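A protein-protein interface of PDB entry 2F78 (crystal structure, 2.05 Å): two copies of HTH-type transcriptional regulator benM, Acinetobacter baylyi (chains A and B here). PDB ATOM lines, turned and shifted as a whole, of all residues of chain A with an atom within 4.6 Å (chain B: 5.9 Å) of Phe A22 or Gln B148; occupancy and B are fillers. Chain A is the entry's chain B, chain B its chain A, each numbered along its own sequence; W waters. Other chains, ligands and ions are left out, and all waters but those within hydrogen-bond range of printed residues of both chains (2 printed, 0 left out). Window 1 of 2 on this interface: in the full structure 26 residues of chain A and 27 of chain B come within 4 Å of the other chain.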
ATOM      1  N   GLY A  18     -21.983  20.361  11.698  1.00  0.00           N
ATOM      2  CA  GLY A  18     -20.602  20.436  12.199  1.00  0.00           C
ATOM      3  C   GLY A  18     -20.098  19.302  13.083  1.00  0.00           C
ATOM      4  O   GLY A  18     -18.936  18.923  13.003  1.00  0.00           O
ATOM      5  N   SER A  19     -20.961  18.753  13.932  1.00  0.00           N
ATOM      6  CA  SER A  19     -20.555  17.661  14.820  1.00  0.00           C
ATOM      7  C   SER A  19     -20.072  16.416  14.058  1.00  0.00           C
ATOM      8  O   SER A  19     -19.296  15.621  14.589  1.00  0.00           O
ATOM      9  CB  SER A  19     -21.679  17.301  15.801  1.00  0.00           C
ATOM     10  OG  SER A  19     -22.815  16.775  15.150  1.00  0.00           O
ATOM     11  N   LEU A  20     -20.506  16.266  12.804  1.00  0.00           N
ATOM     12  CA  LEU A  20     -20.104  15.126  11.976  1.00  0.00           C
ATOM     13  C   LEU A  20     -18.621  15.159  11.556  1.00  0.00           C
ATOM     14  O   LEU A  20     -18.080  14.153  11.112  1.00  0.00           O
ATOM     15  CB  LEU A  20     -21.034  15.004  10.760  1.00  0.00           C
ATOM     16  CG  LEU A  20     -22.522  14.872  11.117  1.00  0.00           C
ATOM     17  CD1 LEU A  20     -23.385  14.777   9.874  1.00  0.00           C
ATOM     18  CD2 LEU A  20     -22.765  13.659  12.014  1.00  0.00           C
ATOM     19  N   LEU A  21     -17.959  16.298  11.730  1.00  0.00           N
ATOM     20  CA  LEU A  21     -16.529  16.418  11.443  1.00  0.00           C
ATOM     21  C   LEU A  21     -15.663  15.660  12.441  1.00  0.00           C
ATOM     22  O   LEU A  21     -14.533  15.289  12.125  1.00  0.00           O
ATOM     23  CB  LEU A  21     -16.108  17.894  11.403  1.00  0.00           C
ATOM     24  CG  LEU A  21     -16.661  18.697  10.218  1.00  0.00           C
ATOM     25  CD1 LEU A  21     -16.235  20.144  10.291  1.00  0.00           C
ATOM     26  CD2 LEU A  21     -16.233  18.082   8.881  1.00  0.00           C
ATOM     27  N   PHE A  22     -16.187  15.420  13.638  1.00  0.00           N
ATOM     28  CA  PHE A  22     -15.478  14.599  14.619  1.00  0.00           C
ATOM     29  C   PHE A  22     -15.648  13.100  14.372  1.00  0.00           C
ATOM     30  O   PHE A  22     -14.927  12.298  14.958  1.00  0.00           O
ATOM     31  CB  PHE A  22     -15.913  14.975  16.033  1.00  0.00           C
ATOM     32  CG  PHE A  22     -15.597  16.389  16.387  1.00  0.00           C
ATOM     33  CD1 PHE A  22     -14.280  16.815  16.451  1.00  0.00           C
ATOM     34  CD2 PHE A  22     -16.610  17.309  16.627  1.00  0.00           C
ATOM     35  CE1 PHE A  22     -13.968  18.123  16.766  1.00  0.00           C
ATOM     36  CE2 PHE A  22     -16.306  18.627  16.941  1.00  0.00           C
ATOM     37  CZ  PHE A  22     -14.981  19.032  17.010  1.00  0.00           C
ATOM     38  N   GLY A  23     -16.580  12.735  13.494  1.00  0.00           N
ATOM     39  CA  GLY A  23     -16.854  11.342  13.160  1.00  0.00           C
ATOM     40  C   GLY A  23     -16.274  10.941  11.819  1.00  0.00           C
ATOM     41  O   GLY A  23     -15.126  11.275  11.508  1.00  0.00           O
ATOM     42  N   GLU A 146     -20.963  26.403  22.081  1.00  0.00           N
ATOM     43  CA  GLU A 146     -20.568  25.262  21.271  1.00  0.00           C
ATOM     44  C   GLU A 146     -19.863  24.203  22.108  1.00  0.00           C
ATOM     45  O   GLU A 146     -19.552  24.418  23.288  1.00  0.00           O
ATOM     46  CB  GLU A 146     -19.667  25.726  20.117  1.00  0.00           C
ATOM     47  CG  GLU A 146     -18.288  26.196  20.585  1.00  0.00           C
ATOM     48  CD  GLU A 146     -17.427  26.761  19.470  1.00  0.00           C
ATOM     49  OE1 GLU A 146     -17.883  26.803  18.298  1.00  0.00           O
ATOM     50  OE2 GLU A 146     -16.283  27.165  19.784  1.00  0.00           O
ATOM     51  N   VAL A 147     -19.610  23.063  21.479  1.00  0.00           N
ATOM     52  CA  VAL A 147     -19.071  21.888  22.164  1.00  0.00           C
ATOM     53  C   VAL A 147     -17.742  22.120  22.885  1.00  0.00           C
ATOM     54  O   VAL A 147     -17.601  21.701  24.044  1.00  0.00           O
ATOM     55  CB  VAL A 147     -18.933  20.670  21.208  1.00  0.00           C
ATOM     56  CG1 VAL A 147     -17.908  20.936  20.087  1.00  0.00           C
ATOM     57  CG2 VAL A 147     -18.573  19.413  22.003  1.00  0.00           C
ATOM     58  N   GLN A 148     -16.774  22.776  22.237  1.00  0.00           N
ATOM     59  CA  GLN A 148     -15.449  22.959  22.871  1.00  0.00           C
ATOM     60  C   GLN A 148     -15.513  23.825  24.117  1.00  0.00           C
ATOM     61  O   GLN A 148     -14.686  23.666  25.021  1.00  0.00           O
ATOM     62  CB  GLN A 148     -14.395  23.526  21.911  1.00  0.00           C
ATOM     63  CG  GLN A 148     -14.816  24.737  21.125  1.00  0.00           C
ATOM     64  CD  GLN A 148     -15.247  24.362  19.726  1.00  0.00           C
ATOM     65  OE1 GLN A 148     -16.343  23.836  19.521  1.00  0.00           O
ATOM     66  NE2 GLN A 148     -14.380  24.627  18.750  1.00  0.00           N
ATOM     67  N   SER A 166     -18.323  10.452  19.307  1.00  0.00           N
ATOM     68  CA  SER A 166     -17.217  10.950  18.468  1.00  0.00           C
ATOM     69  C   SER A 166     -16.563  12.230  19.020  1.00  0.00           C
ATOM     70  O   SER A 166     -15.476  12.616  18.600  1.00  0.00           O
ATOM     71  CB  SER A 166     -17.713  11.195  17.052  1.00  0.00           C
ATOM     72  OG  SER A 166     -18.752  12.156  17.062  1.00  0.00           O
ATOM     73  N   SER A 169     -12.746  12.569  20.159  1.00  0.00           N
ATOM     74  CA  SER A 169     -11.653  13.138  19.366  1.00  0.00           C
ATOM     75  C   SER A 169     -10.975  14.299  20.090  1.00  0.00           C
ATOM     76  O   SER A 169      -9.809  14.581  19.866  1.00  0.00           O
ATOM     77  CB  SER A 169     -12.179  13.622  18.027  1.00  0.00           C
ATOM     78  OG  SER A 169     -12.729  12.548  17.290  1.00  0.00           O
ATOM     79  N   ILE A 170     -11.726  14.981  20.944  1.00  0.00           N
ATOM     80  CA  ILE A 170     -11.171  16.049  21.764  1.00  0.00           C
ATOM     81  C   ILE A 170     -10.776  15.486  23.117  1.00  0.00           C
ATOM     82  O   ILE A 170     -11.630  15.047  23.884  1.00  0.00           O
ATOM     83  CB  ILE A 170     -12.170  17.195  21.951  1.00  0.00           C
ATOM     84  CG1 ILE A 170     -12.652  17.693  20.580  1.00  0.00           C
ATOM     85  CG2 ILE A 170     -11.528  18.308  22.811  1.00  0.00           C
ATOM     86  CD1 ILE A 170     -13.692  18.801  20.627  1.00  0.00           C
ATOM     87  N   ARG B 145     -14.883  29.091   9.052  1.00  0.00           N
ATOM     88  CA  ARG B 145     -15.552  29.610  10.251  1.00  0.00           C
ATOM     89  C   ARG B 145     -14.718  29.530  11.529  1.00  0.00           C
ATOM     90  O   ARG B 145     -14.542  30.537  12.217  1.00  0.00           O
ATOM     91  CB  ARG B 145     -16.888  28.891  10.471  1.00  0.00           C
ATOM     92  CG  ARG B 145     -17.851  29.667  11.337  1.00  0.00           C
ATOM     93  CD  ARG B 145     -19.235  29.062  11.284  1.00  0.00           C
ATOM     94  NE  ARG B 145     -19.272  27.761  11.943  1.00  0.00           N
ATOM     95  CZ  ARG B 145     -19.429  27.580  13.253  1.00  0.00           C
ATOM     96  NH1 ARG B 145     -19.537  28.616  14.080  1.00  0.00           N
ATOM     97  NH2 ARG B 145     -19.460  26.348  13.741  1.00  0.00           N
ATOM     98  N   GLU B 146     -14.235  28.337  11.862  1.00  0.00           N
ATOM     99  CA  GLU B 146     -13.412  28.154  13.058  1.00  0.00           C
ATOM    100  C   GLU B 146     -12.552  26.885  12.996  1.00  0.00           C
ATOM    101  O   GLU B 146     -12.608  26.138  12.020  1.00  0.00           O
ATOM    102  CB  GLU B 146     -14.284  28.189  14.322  1.00  0.00           C
ATOM    103  CG  GLU B 146     -15.368  27.157  14.370  1.00  0.00           C
ATOM    104  CD  GLU B 146     -16.262  27.284  15.610  1.00  0.00           C
ATOM    105  OE1 GLU B 146     -15.914  28.024  16.564  1.00  0.00           O
ATOM    106  OE2 GLU B 146     -17.335  26.654  15.621  1.00  0.00           O
ATOM    107  N   VAL B 147     -11.762  26.658  14.045  1.00  0.00           N
ATOM    108  CA  VAL B 147     -10.685  25.673  14.013  1.00  0.00           C
ATOM    109  C   VAL B 147     -11.115  24.266  13.595  1.00  0.00           C
ATOM    110  O   VAL B 147     -10.453  23.637  12.755  1.00  0.00           O
ATOM    111  CB  VAL B 147      -9.920  25.616  15.358  1.00  0.00           C
ATOM    112  CG1 VAL B 147     -10.802  25.075  16.490  1.00  0.00           C
ATOM    113  CG2 VAL B 147      -8.649  24.795  15.199  1.00  0.00           C
ATOM    114  N   GLN B 148     -12.216  23.775  14.158  1.00  0.00           N
ATOM    115  CA  GLN B 148     -12.607  22.385  13.914  1.00  0.00           C
ATOM    116  C   GLN B 148     -13.117  22.179  12.497  1.00  0.00           C
ATOM    117  O   GLN B 148     -13.010  21.084  11.948  1.00  0.00           O
ATOM    118  CB  GLN B 148     -13.611  21.884  14.956  1.00  0.00           C
ATOM    119  CG  GLN B 148     -15.036  22.363  14.781  1.00  0.00           C
ATOM    120  CD  GLN B 148     -15.289  23.763  15.309  1.00  0.00           C
ATOM    121  OE1 GLN B 148     -14.475  24.336  16.045  1.00  0.00           O
ATOM    122  NE2 GLN B 148     -16.446  24.317  14.944  1.00  0.00           N
ATOM    123  N   LEU B 149     -13.683  23.226  11.909  1.00  0.00           N
ATOM    124  CA  LEU B 149     -14.036  23.191  10.502  1.00  0.00           C
ATOM    125  C   LEU B 149     -12.762  23.075   9.673  1.00  0.00           C
ATOM    126  O   LEU B 149     -12.709  22.307   8.718  1.00  0.00           O
ATOM    127  CB  LEU B 149     -14.833  24.438  10.106  1.00  0.00           C
ATOM    128  CG  LEU B 149     -15.396  24.470   8.684  1.00  0.00           C
ATOM    129  CD1 LEU B 149     -16.092  23.163   8.315  1.00  0.00           C
ATOM    130  CD2 LEU B 149     -16.350  25.634   8.531  1.00  0.00           C
ATOM    131  N   ALA B 150     -11.726  23.827  10.057  1.00  0.00           N
ATOM    132  CA  ALA B 150     -10.439  23.769   9.360  1.00  0.00           C
ATOM    133  C   ALA B 150      -9.840  22.366   9.443  1.00  0.00           C
ATOM    134  O   ALA B 150      -9.435  21.810   8.430  1.00  0.00           O
ATOM    135  CB  ALA B 150      -9.454  24.813   9.914  1.00  0.00           C
ATOM    136  N   LEU B 151      -9.821  21.794  10.640  1.00  0.00           N
ATOM    137  CA  LEU B 151      -9.248  20.471  10.851  1.00  0.00           C
ATOM    138  C   LEU B 151     -10.037  19.378  10.132  1.00  0.00           C
ATOM    139  O   LEU B 151      -9.443  18.485   9.537  1.00  0.00           O
ATOM    140  CB  LEU B 151      -9.196  20.147  12.343  1.00  0.00           C
ATOM    141  CG  LEU B 151      -8.366  21.075  13.234  1.00  0.00           C
ATOM    142  CD1 LEU B 151      -8.559  20.663  14.666  1.00  0.00           C
ATOM    143  CD2 LEU B 151      -6.895  21.042  12.843  1.00  0.00           C
ATOM    144  N   GLY B 152     -11.369  19.454  10.202  1.00  0.00           N
ATOM    145  CA  GLY B 152     -12.252  18.531   9.480  1.00  0.00           C
ATOM    146  C   GLY B 152     -11.978  18.526   7.988  1.00  0.00           C
ATOM    147  O   GLY B 152     -11.916  17.459   7.365  1.00  0.00           O
ATOM    148  N   LEU B 153     -11.806  19.716   7.420  1.00  0.00           N
ATOM    149  CA  LEU B 153     -11.512  19.857   5.998  1.00  0.00           C
ATOM    150  C   LEU B 153     -10.114  19.342   5.648  1.00  0.00           C
ATOM    151  O   LEU B 153      -9.917  18.766   4.590  1.00  0.00           O
ATOM    152  CB  LEU B 153     -11.670  21.313   5.557  1.00  0.00           C
ATOM    153  CG  LEU B 153     -13.084  21.891   5.648  1.00  0.00           C
ATOM    154  CD1 LEU B 153     -13.030  23.393   5.456  1.00  0.00           C
ATOM    155  CD2 LEU B 153     -14.012  21.251   4.632  1.00  0.00           C
ATOM    156  N   ILE B 170      -7.083  17.958  19.775  1.00  0.00           N
ATOM    157  CA  ILE B 170      -7.999  17.374  18.815  1.00  0.00           C
ATOM    158  C   ILE B 170      -7.234  16.421  17.924  1.00  0.00           C
ATOM    159  O   ILE B 170      -6.331  16.832  17.179  1.00  0.00           O
ATOM    160  CB  ILE B 170      -8.693  18.449  17.953  1.00  0.00           C
ATOM    161  CG1 ILE B 170      -9.361  19.490  18.856  1.00  0.00           C
ATOM    162  CG2 ILE B 170      -9.718  17.810  17.022  1.00  0.00           C
ATOM    163  CD1 ILE B 170      -9.719  20.771  18.155  1.00  0.00           C
ATOM    164  N   LEU B 172      -8.045  13.704  14.973  1.00  0.00           N
ATOM    165  CA  LEU B 172      -8.993  13.137  14.015  1.00  0.00           C
ATOM    166  C   LEU B 172      -8.311  12.075  13.182  1.00  0.00           C
ATOM    167  O   LEU B 172      -7.090  12.104  13.007  1.00  0.00           O
ATOM    168  CB  LEU B 172      -9.509  14.217  13.072  1.00  0.00           C
ATOM    169  CG  LEU B 172     -10.163  15.437  13.711  1.00  0.00           C
ATOM    170  CD1 LEU B 172     -10.617  16.379  12.611  1.00  0.00           C
ATOM    171  CD2 LEU B 172     -11.331  15.034  14.589  1.00  0.00           C
HETATM  172  O   HOH W   1     -17.980  23.144  17.589  1.00  0.00           O
HETATM  173  O   HOH W   2     -19.800  27.156  16.897  1.00  0.00           O
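Of the printed residues of chain B, Glu A146 touches Glu B146. Ile A170 touches none of the printed residues of chain B. Of chain A, only Leu A21 (3.7 Å), Phe A22 (3.8 Å) and Gln A148 (2.7 Å) come within 4 Å of Gln B148. Printed residues of chain A within 4 Å of Leu B149: Leu A21 (3.6 Å). Printed residues of chain A within 4 Å of Ile B170: Ser A169. The nearest residue of chain B that does not touch Phe A22 is Ile B170 (4.3 Å). The nearest residue of chain A that does not touch Gln B148 is Glu A146 (4.4 Å).
OE1 of Glu A146 lies close to OE2 of Glu B146 (2.7 Å). OE1 of Gln B148 is in hydrogen-bond range of NE2 of Gln A148 (2.7 Å).
Water W2 lies within hydrogen-bond range of OE1 of Glu A146 (2.4 Å), OE2 of Glu B146 (2.8 Å) and NH1 of Arg B145 (3.2 Å). Water W1 lies within hydrogen-bond range of the side-chain amide oxygen of Gln A148 and the side-chain amide nitrogen of Gln B148.
Glu A146 touches its own counterpart, Glu B146. Gln B148 touches its own counterpart, Gln A148. 4 positions are printed for both chains. Of the 8 pairs that touch across the chains among the printed residues, 2 have their exchanged pair printed and touching as well.
The backbone carbonyl oxygen of Ser A166 is in hydrogen-bond range of the side-chain hydroxyl of Ser A169, at 3.0 Å. NE2 of Gln B148 sits at hydrogen-bond distance from OE2 of Glu B146, 2.6 Å away. NE2 of Gln A148 sits close to OE2 of Glu A146, at 3.3 Å. NH2 of Arg B145 lies within salt-bridge range of OE2 of Glu B146, 2.9 Å away. The backbone carbonyl oxygen of Phe A22 lies within hydrogen-bond range of the side-chain hydroxyl of Ser A169, at 3.2 Å.
Of the 12 printed residues of chain A, 5 touch a printed residue of chain B. Among the printed residues, no Asp or Glu carboxylate lies within 4 Å of a Lys or Arg side-chain nitrogen of the other chain.
Among the printed residues, merely in contact across the chains: Leu A21 with Gln B148 (3.7 Å), Leu A21 with Leu B149 (3.6 Å), Phe A22 with Gln B148 (3.8 Å), Phe A22 with Leu B172 (3.9 Å), Ser A169 with Ile B170 (3.5 Å) and Ser A169 with Leu B172 (3.8 Å).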
